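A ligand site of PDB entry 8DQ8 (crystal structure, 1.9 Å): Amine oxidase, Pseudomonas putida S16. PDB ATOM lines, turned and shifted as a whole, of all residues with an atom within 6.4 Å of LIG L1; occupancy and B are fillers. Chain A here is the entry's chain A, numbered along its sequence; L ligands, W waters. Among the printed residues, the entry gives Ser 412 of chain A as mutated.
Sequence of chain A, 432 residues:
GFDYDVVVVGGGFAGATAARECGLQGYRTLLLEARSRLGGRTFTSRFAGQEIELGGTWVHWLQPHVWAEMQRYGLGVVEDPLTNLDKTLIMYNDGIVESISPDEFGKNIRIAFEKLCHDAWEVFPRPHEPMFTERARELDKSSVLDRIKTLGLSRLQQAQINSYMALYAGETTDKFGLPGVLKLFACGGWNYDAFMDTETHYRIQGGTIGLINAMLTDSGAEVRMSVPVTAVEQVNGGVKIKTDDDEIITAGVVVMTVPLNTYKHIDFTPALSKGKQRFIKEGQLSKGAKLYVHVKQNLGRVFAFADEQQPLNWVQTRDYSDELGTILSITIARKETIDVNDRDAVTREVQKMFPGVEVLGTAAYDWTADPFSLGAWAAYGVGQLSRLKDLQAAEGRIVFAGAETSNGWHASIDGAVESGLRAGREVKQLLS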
ATOM      1  N   TRP A  58      -3.317  25.860  17.816  1.00  0.00           N
ATOM      2  CA  TRP A  58      -2.892  24.463  17.778  1.00  0.00           C
ATOM      3  C   TRP A  58      -1.501  24.315  17.132  1.00  0.00           C
ATOM      4  O   TRP A  58      -1.131  25.084  16.221  1.00  0.00           O
ATOM      5  CB  TRP A  58      -3.898  23.604  16.991  1.00  0.00           C
ATOM      6  CG  TRP A  58      -5.281  23.567  17.588  1.00  0.00           C
ATOM      7  CD1 TRP A  58      -5.686  22.839  18.689  1.00  0.00           C
ATOM      8  CD2 TRP A  58      -6.436  24.263  17.108  1.00  0.00           C
ATOM      9  NE1 TRP A  58      -7.060  23.062  18.933  1.00  0.00           N
ATOM     10  CE2 TRP A  58      -7.517  23.924  17.957  1.00  0.00           C
ATOM     11  CE3 TRP A  58      -6.660  25.147  16.036  1.00  0.00           C
ATOM     12  CZ2 TRP A  58      -8.819  24.474  17.794  1.00  0.00           C
ATOM     13  CZ3 TRP A  58      -7.976  25.652  15.836  1.00  0.00           C
ATOM     14  CH2 TRP A  58      -9.020  25.318  16.728  1.00  0.00           C
ATOM     15  N   TYR A 164     -12.250  24.529   3.433  1.00  0.00           N
ATOM     16  CA  TYR A 164     -10.909  24.481   4.027  1.00  0.00           C
ATOM     17  C   TYR A 164     -10.009  25.573   3.455  1.00  0.00           C
ATOM     18  O   TYR A 164      -9.292  26.268   4.190  1.00  0.00           O
ATOM     19  CB  TYR A 164     -10.301  23.091   3.740  1.00  0.00           C
ATOM     20  CG  TYR A 164      -9.246  22.549   4.695  1.00  0.00           C
ATOM     21  CD1 TYR A 164      -8.103  23.282   5.029  1.00  0.00           C
ATOM     22  CD2 TYR A 164      -9.368  21.256   5.210  1.00  0.00           C
ATOM     23  CE1 TYR A 164      -7.139  22.746   5.940  1.00  0.00           C
ATOM     24  CE2 TYR A 164      -8.415  20.725   6.103  1.00  0.00           C
ATOM     25  CZ  TYR A 164      -7.295  21.447   6.422  1.00  0.00           C
ATOM     26  OH  TYR A 164      -6.376  20.846   7.343  1.00  0.00           O
ATOM     27  N   LEU A 167     -10.984  29.199   4.418  1.00  0.00           N
ATOM     28  CA  LEU A 167     -10.427  29.461   5.762  1.00  0.00           C
ATOM     29  C   LEU A 167      -8.939  29.795   5.669  1.00  0.00           C
ATOM     30  O   LEU A 167      -8.496  30.840   6.185  1.00  0.00           O
ATOM     31  CB  LEU A 167     -10.645  28.245   6.671  1.00  0.00           C
ATOM     32  CG  LEU A 167     -10.525  28.420   8.204  1.00  0.00           C
ATOM     33  CD1 LEU A 167      -9.113  28.516   8.619  1.00  0.00           C
ATOM     34  CD2 LEU A 167     -11.343  29.690   8.688  1.00  0.00           C
ATOM     35  N   TYR A 168      -8.135  28.956   4.986  1.00  0.00           N
ATOM     36  CA  TYR A 168      -6.698  29.287   4.965  1.00  0.00           C
ATOM     37  C   TYR A 168      -6.407  30.585   4.202  1.00  0.00           C
ATOM     38  O   TYR A 168      -5.401  31.259   4.493  1.00  0.00           O
ATOM     39  CB  TYR A 168      -5.833  28.097   4.419  1.00  0.00           C
ATOM     40  CG  TYR A 168      -5.568  27.140   5.597  1.00  0.00           C
ATOM     41  CD1 TYR A 168      -6.641  26.539   6.286  1.00  0.00           C
ATOM     42  CD2 TYR A 168      -4.266  26.950   6.121  1.00  0.00           C
ATOM     43  CE1 TYR A 168      -6.422  25.719   7.429  1.00  0.00           C
ATOM     44  CE2 TYR A 168      -4.058  26.121   7.236  1.00  0.00           C
ATOM     45  CZ  TYR A 168      -5.141  25.519   7.876  1.00  0.00           C
ATOM     46  OH  TYR A 168      -4.924  24.720   8.989  1.00  0.00           O
ATOM     47  N   THR A 198      -1.676  18.150  12.118  1.00  0.00           N
ATOM     48  CA  THR A 198      -0.884  19.271  12.616  1.00  0.00           C
ATOM     49  C   THR A 198      -1.736  20.525  12.842  1.00  0.00           C
ATOM     50  O   THR A 198      -1.241  21.485  13.432  1.00  0.00           O
ATOM     51  CB  THR A 198       0.242  19.685  11.655  1.00  0.00           C
ATOM     52  OG1 THR A 198      -0.348  20.276  10.466  1.00  0.00           O
ATOM     53  CG2 THR A 198       1.198  18.487  11.306  1.00  0.00           C
ATOM     54  N   GLU A 199      -2.951  20.587  12.345  1.00  0.00           N
ATOM     55  CA  GLU A 199      -3.595  21.891  12.223  1.00  0.00           C
ATOM     56  C   GLU A 199      -4.552  22.243  13.362  1.00  0.00           C
ATOM     57  O   GLU A 199      -4.586  23.401  13.746  1.00  0.00           O
ATOM     58  CB  GLU A 199      -4.364  21.972  10.894  1.00  0.00           C
ATOM     59  CG  GLU A 199      -3.376  21.992   9.692  1.00  0.00           C
ATOM     60  CD  GLU A 199      -2.289  23.056   9.859  1.00  0.00           C
ATOM     61  OE1 GLU A 199      -2.594  24.277   9.601  1.00  0.00           O
ATOM     62  OE2 GLU A 199      -1.141  22.719  10.252  1.00  0.00           O
ATOM     63  N   THR A 200      -5.365  21.302  13.874  1.00  0.00           N
ATOM     64  CA  THR A 200      -6.351  21.730  14.894  1.00  0.00           C
ATOM     65  C   THR A 200      -6.525  20.698  16.006  1.00  0.00           C
ATOM     66  O   THR A 200      -7.597  20.651  16.645  1.00  0.00           O
ATOM     67  CB  THR A 200      -7.749  22.035  14.286  1.00  0.00           C
ATOM     68  OG1 THR A 200      -8.403  20.829  13.854  1.00  0.00           O
ATOM     69  CG2 THR A 200      -7.643  23.042  13.106  1.00  0.00           C
ATOM     70  N   LYS A 290     -12.348  35.025  14.976  1.00  0.00           N
ATOM     71  CA  LYS A 290     -12.552  33.771  15.700  1.00  0.00           C
ATOM     72  C   LYS A 290     -13.514  34.007  16.852  1.00  0.00           C
ATOM     73  O   LYS A 290     -13.544  35.105  17.430  1.00  0.00           O
ATOM     74  CB  LYS A 290     -11.209  33.214  16.253  1.00  0.00           C
ATOM     75  CG  LYS A 290     -11.343  31.838  16.884  1.00  0.00           C
ATOM     76  CD  LYS A 290      -9.944  31.168  17.030  1.00  0.00           C
ATOM     77  CE  LYS A 290     -10.116  29.791  17.730  1.00  0.00           C
ATOM     78  NZ  LYS A 290      -8.752  29.183  18.116  1.00  0.00           N
ATOM     79  N   TRP A 314     -15.282  26.948  10.015  1.00  0.00           N
ATOM     80  CA  TRP A 314     -14.588  25.795  10.634  1.00  0.00           C
ATOM     81  C   TRP A 314     -15.049  25.720  12.080  1.00  0.00           C
ATOM     82  O   TRP A 314     -14.738  26.629  12.880  1.00  0.00           O
ATOM     83  CB  TRP A 314     -13.073  25.976  10.538  1.00  0.00           C
ATOM     84  CG  TRP A 314     -12.289  24.819  11.058  1.00  0.00           C
ATOM     85  CD1 TRP A 314     -12.319  24.284  12.306  1.00  0.00           C
ATOM     86  CD2 TRP A 314     -11.349  24.048  10.307  1.00  0.00           C
ATOM     87  NE1 TRP A 314     -11.434  23.188  12.387  1.00  0.00           N
ATOM     88  CE2 TRP A 314     -10.813  23.065  11.167  1.00  0.00           C
ATOM     89  CE3 TRP A 314     -10.872  24.132   8.989  1.00  0.00           C
ATOM     90  CZ2 TRP A 314      -9.834  22.145  10.737  1.00  0.00           C
ATOM     91  CZ3 TRP A 314      -9.886  23.234   8.578  1.00  0.00           C
ATOM     92  CH2 TRP A 314      -9.389  22.258   9.466  1.00  0.00           C
ATOM     93  N   GLN A 316     -15.380  23.219  15.613  1.00  0.00           N
ATOM     94  CA  GLN A 316     -15.100  21.972  16.314  1.00  0.00           C
ATOM     95  C   GLN A 316     -15.341  22.156  17.805  1.00  0.00           C
ATOM     96  O   GLN A 316     -15.587  23.268  18.302  1.00  0.00           O
ATOM     97  CB  GLN A 316     -13.645  21.463  15.998  1.00  0.00           C
ATOM     98  CG  GLN A 316     -12.540  22.427  16.305  1.00  0.00           C
ATOM     99  CD  GLN A 316     -11.151  21.836  15.953  1.00  0.00           C
ATOM    100  OE1 GLN A 316     -10.853  21.527  14.779  1.00  0.00           O
ATOM    101  NE2 GLN A 316     -10.321  21.655  16.986  1.00  0.00           N
ATOM    102  N   SER A 329     -15.471  25.964  19.282  1.00  0.00           N
ATOM    103  CA  SER A 329     -14.476  26.858  18.715  1.00  0.00           C
ATOM    104  C   SER A 329     -14.834  27.050  17.233  1.00  0.00           C
ATOM    105  O   SER A 329     -14.943  26.060  16.497  1.00  0.00           O
ATOM    106  CB  SER A 329     -13.070  26.227  18.818  1.00  0.00           C
ATOM    107  OG  SER A 329     -12.092  27.034  18.093  1.00  0.00           O
ATOM    108  N   ILE A 330     -14.991  28.301  16.793  1.00  0.00           N
ATOM    109  CA  ILE A 330     -15.435  28.611  15.458  1.00  0.00           C
ATOM    110  C   ILE A 330     -14.464  29.602  14.863  1.00  0.00           C
ATOM    111  O   ILE A 330     -14.248  30.679  15.444  1.00  0.00           O
ATOM    112  CB  ILE A 330     -16.870  29.201  15.432  1.00  0.00           C
ATOM    113  CG1 ILE A 330     -17.891  28.257  16.117  1.00  0.00           C
ATOM    114  CG2 ILE A 330     -17.299  29.530  13.971  1.00  0.00           C
ATOM    115  CD1 ILE A 330     -19.394  28.728  16.045  1.00  0.00           C
ATOM    116  N   THR A 331     -13.896  29.269  13.698  1.00  0.00           N
ATOM    117  CA  THR A 331     -13.060  30.209  12.968  1.00  0.00           C
ATOM    118  C   THR A 331     -13.780  30.657  11.695  1.00  0.00           C
ATOM    119  O   THR A 331     -14.352  29.837  10.955  1.00  0.00           O
ATOM    120  CB  THR A 331     -11.663  29.627  12.624  1.00  0.00           C
ATOM    121  OG1 THR A 331     -11.123  29.005  13.793  1.00  0.00           O
ATOM    122  CG2 THR A 331     -10.700  30.779  12.171  1.00  0.00           C
ATOM    123  N   TRP A 377      -4.239  35.223  10.178  1.00  0.00           N
ATOM    124  CA  TRP A 377      -3.032  34.457   9.783  1.00  0.00           C
ATOM    125  C   TRP A 377      -2.533  34.883   8.404  1.00  0.00           C
ATOM    126  O   TRP A 377      -3.280  35.362   7.543  1.00  0.00           O
ATOM    127  CB  TRP A 377      -3.356  32.951   9.750  1.00  0.00           C
ATOM    128  CG  TRP A 377      -4.615  32.721   8.991  1.00  0.00           C
ATOM    129  CD1 TRP A 377      -4.735  32.536   7.632  1.00  0.00           C
ATOM    130  CD2 TRP A 377      -5.948  32.752   9.527  1.00  0.00           C
ATOM    131  NE1 TRP A 377      -6.061  32.468   7.301  1.00  0.00           N
ATOM    132  CE2 TRP A 377      -6.824  32.603   8.447  1.00  0.00           C
ATOM    133  CE3 TRP A 377      -6.473  32.905  10.819  1.00  0.00           C
ATOM    134  CZ2 TRP A 377      -8.244  32.610   8.602  1.00  0.00           C
ATOM    135  CZ3 TRP A 377      -7.877  32.915  10.981  1.00  0.00           C
ATOM    136  CH2 TRP A 377      -8.742  32.732   9.889  1.00  0.00           C
ATOM    137  N   ALA A 378      -1.237  34.640   8.155  1.00  0.00           N
ATOM    138  CA  ALA A 378      -0.664  34.991   6.855  1.00  0.00           C
ATOM    139  C   ALA A 378      -1.295  34.167   5.739  1.00  0.00           C
ATOM    140  O   ALA A 378      -1.348  32.936   5.843  1.00  0.00           O
ATOM    141  CB  ALA A 378       0.853  34.747   6.869  1.00  0.00           C
ATOM    142  N   ALA A 411       1.706  30.132   7.945  1.00  0.00           N
ATOM    143  CA  ALA A 411       0.359  30.441   8.478  1.00  0.00           C
ATOM    144  C   ALA A 411       0.245  30.131   9.952  1.00  0.00           C
ATOM    145  O   ALA A 411      -0.886  30.097  10.490  1.00  0.00           O
ATOM    146  CB  ALA A 411      -0.705  29.650   7.721  1.00  0.00           C
ATOM    147  N   SER A 412       1.378  29.923  10.642  1.00  0.00           N
ATOM    148  CA  SER A 412       1.386  29.235  11.946  1.00  0.00           C
ATOM    149  C   SER A 412       2.235  29.962  13.001  1.00  0.00           C
ATOM    150  O   SER A 412       3.034  30.846  12.697  1.00  0.00           O
ATOM    151  CB  SER A 412       1.952  27.807  11.780  1.00  0.00           C
ATOM    152  OG  SER A 412       1.343  27.144  10.698  1.00  0.00           O
HETATM  153  N1  LIG L   1      -8.998  27.571  12.741  1.00  0.00           N
HETATM  154  C1  LIG L   1      -7.804  28.093  12.478  1.00  0.00           C
HETATM  155  C2  LIG L   1      -6.923  27.391  11.676  1.00  0.00           C
HETATM  156  C3  LIG L   1      -7.253  26.143  11.141  1.00  0.00           C
HETATM  157  C4  LIG L   1      -8.511  25.646  11.436  1.00  0.00           C
HETATM  158  C5  LIG L   1      -9.354  26.404  12.219  1.00  0.00           C
HETATM  159  N2  LIG L   1      -4.357  27.268  11.513  1.00  0.00           N
HETATM  160  C6  LIG L   1      -5.580  27.990  11.383  1.00  0.00           C
HETATM  161  C7  LIG L   1      -5.368  29.092  10.344  1.00  0.00           C
HETATM  162  C8  LIG L   1      -3.956  29.389  10.389  1.00  0.00           C
HETATM  163  C9  LIG L   1      -3.262  28.123  10.907  1.00  0.00           C
HETATM  164  C10 LIG L   1      -4.171  25.977  12.142  1.00  0.00           C
HETATM  165  P1  LG2 L   2       2.063  38.860  15.772  1.00  0.00           P
HETATM  166  O1  LG2 L   2       0.994  39.634  14.989  1.00  0.00           O
HETATM  167  O2  LG2 L   2       1.703  37.733  16.708  1.00  0.00           O
HETATM  168  O3  LG2 L   2       3.045  39.823  16.572  1.00  0.00           O
HETATM  169  C1  LG2 L   2       3.291  41.095  16.002  1.00  0.00           C
HETATM  170  C2  LG2 L   2       3.274  42.100  17.150  1.00  0.00           C
HETATM  171  O4  LG2 L   2       3.560  43.436  16.693  1.00  0.00           O
HETATM  172  C3  LG2 L   2       1.855  42.157  17.793  1.00  0.00           C
HETATM  173  O5  LG2 L   2       1.931  41.875  19.179  1.00  0.00           O
HETATM  174  C4  LG2 L   2       1.415  43.628  17.527  1.00  0.00           C
HETATM  175  O6  LG2 L   2       0.672  44.199  18.569  1.00  0.00           O
HETATM  176  C5  LG2 L   2       2.741  44.364  17.418  1.00  0.00           C
HETATM  177  N1  LG2 L   2       2.756  45.614  16.700  1.00  0.00           N
HETATM  178  C6  LG2 L   2       2.138  45.920  15.521  1.00  0.00           C
HETATM  179  N2  LG2 L   2       2.398  47.171  15.112  1.00  0.00           N
HETATM  180  C7  LG2 L   2       3.258  47.665  16.056  1.00  0.00           C
HETATM  181  C8  LG2 L   2       3.921  48.920  16.210  1.00  0.00           C
HETATM  182  N3  LG2 L   2       3.790  49.902  15.322  1.00  0.00           N
HETATM  183  N4  LG2 L   2       4.725  49.115  17.263  1.00  0.00           N
HETATM  184  C9  LG2 L   2       4.851  48.124  18.152  1.00  0.00           C
HETATM  185  N5  LG2 L   2       4.305  46.888  18.087  1.00  0.00           N
HETATM  186  C10 LG2 L   2       3.496  46.735  17.045  1.00  0.00           C
HETATM  187  N6  LG2 L   2      -1.182  29.425  14.075  1.00  0.00           N
HETATM  188  C11 LG2 L   2      -0.907  28.159  14.543  1.00  0.00           C
HETATM  189  O7  LG2 L   2       0.244  27.670  14.592  1.00  0.00           O
HETATM  190  N7  LG2 L   2      -2.031  27.475  14.938  1.00  0.00           N
HETATM  191  C12 LG2 L   2      -3.360  27.932  14.924  1.00  0.00           C
HETATM  192  O8  LG2 L   2      -4.292  27.245  15.363  1.00  0.00           O
HETATM  193  C13 LG2 L   2      -3.524  29.247  14.393  1.00  0.00           C
HETATM  194  N8  LG2 L   2      -4.808  29.757  14.279  1.00  0.00           N
HETATM  195  C14 LG2 L   2      -4.904  31.143  14.120  1.00  0.00           C
HETATM  196  C15 LG2 L   2      -6.119  31.773  14.387  1.00  0.00           C
HETATM  197  C16 LG2 L   2      -6.268  33.148  14.321  1.00  0.00           C
HETATM  198  C17 LG2 L   2      -7.647  33.757  14.590  1.00  0.00           C
HETATM  199  C18 LG2 L   2      -5.160  33.915  13.989  1.00  0.00           C
HETATM  200  C19 LG2 L   2      -5.272  35.433  13.902  1.00  0.00           C
HETATM  201  C20 LG2 L   2      -3.944  33.277  13.752  1.00  0.00           C
HETATM  202  C21 LG2 L   2      -3.796  31.902  13.819  1.00  0.00           C
HETATM  203  N9  LG2 L   2      -2.555  31.268  13.567  1.00  0.00           N
HETATM  204  C22 LG2 L   2      -2.440  29.974  14.016  1.00  0.00           C
HETATM  205  C23 LG2 L   2      -1.352  32.017  13.146  1.00  0.00           C
HETATM  206  C24 LG2 L   2      -0.442  32.459  14.295  1.00  0.00           C
HETATM  207  O9  LG2 L   2      -1.229  32.928  15.358  1.00  0.00           O
HETATM  208  C25 LG2 L   2       0.523  33.520  13.731  1.00  0.00           C
HETATM  209  O10 LG2 L   2       1.184  33.051  12.581  1.00  0.00           O
HETATM  210  C26 LG2 L   2       1.552  34.078  14.733  1.00  0.00           C
HETATM  211  O11 LG2 L   2       0.959  34.234  15.977  1.00  0.00           O
HETATM  212  C27 LG2 L   2       2.199  35.377  14.217  1.00  0.00           C
HETATM  213  O12 LG2 L   2       3.250  35.705  15.086  1.00  0.00           O
HETATM  214  P2  LG2 L   2       4.124  37.041  14.719  1.00  0.00           P
HETATM  215  O13 LG2 L   2       4.995  37.260  15.910  1.00  0.00           O
HETATM  216  O14 LG2 L   2       4.640  36.889  13.306  1.00  0.00           O
HETATM  217  O15 LG2 L   2       3.039  38.268  14.593  1.00  0.00           O
HETATM  218  O   HOH W   1      -0.857  25.762  11.539  1.00  0.00           O
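An oxygen (O8) of LG2 L2 is in hydrogen-bond range of the backbone NH (N) of Trp 58, 3.0 Å away. The backbone carbonyl oxygen (O) of Trp 58 sits at hydrogen-bond distance from a nitrogen (N7) of LG2 L2. N2 of LIG L1 lies within salt-bridge range of OE1 of Glu 199 (3.96 Å). The backbone carbonyl oxygen (O) of Ser 412 sits at hydrogen-bond distance from an oxygen (O10) of LG2 L2 (2.9 Å). A nitrogen (N1) of LIG L1 is in hydrogen-bond range of the side-chain hydroxyl (OG1) of Thr 331 (2.8 Å).
CZ3 of Trp 58 touches N1 of LIG L1, 3.8 Å away. Leu 167 touches LIG L1. Tyr 168 touches LIG L1 (OH to C3, 3.5 Å). Thr 200 touches LIG L1 (CG2 to C4, 3.2 Å). CD2 of Trp 314 touches C4 of LIG L1, at 3.4 Å. Trp 377 touches LIG L1 (CB to C8, 3.7 Å). Ala 411 touches LIG L1. Hydrophobic or aromatic side chains within 4 Å of LIG L1: Trp 58, Leu 167, Tyr 168, Trp 314 and Trp 377. Nine residues have an atom within 4 Å of LIG L1: Trp 58, Leu 167, Tyr 168, Glu 199, Thr 200, Trp 314, Thr 331, Trp 377 and Ala 411. Along chain A the residues within 4 Å of LIG L1 span positions 58 to 411. The nearest printed residue that does not touch LIG L1 is Ser 412 (4.7 Å).
Water W1 bridges OG of Ser 412 (2.7 Å) and OE1 of Glu 199 (3.0 Å).
The backbone carbonyl oxygen (O) of Tyr 168 lies within hydrogen-bond range of the indole nitrogen (NE1) of Trp 377. The indole nitrogen (NE1) of Trp 377 lies close to the backbone carbonyl oxygen (O) of Leu 167, 3.1 Å away. OE1 of Glu 199 sits at hydrogen-bond distance from OH of Tyr 168. The side-chain amide oxygen (OE1) of Gln 316 lies within hydrogen-bond range of the indole nitrogen (NE1) of Trp 314, at 3.0 Å. O of Trp 314 sits at hydrogen-bond distance from N of Thr 331, at 2.9 Å. The indole nitrogen (NE1) of Trp 58 sits at hydrogen-bond distance from the backbone carbonyl oxygen (O) of Thr 200, at 3.4 Å. OE1 of Gln 316 is in hydrogen-bond range of OG1 of Thr 200. The side-chain hydroxyl (OG1) of Thr 198 is in hydrogen-bond range of the side-chain carboxylate (OE2) of Glu 199 (2.6 Å).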
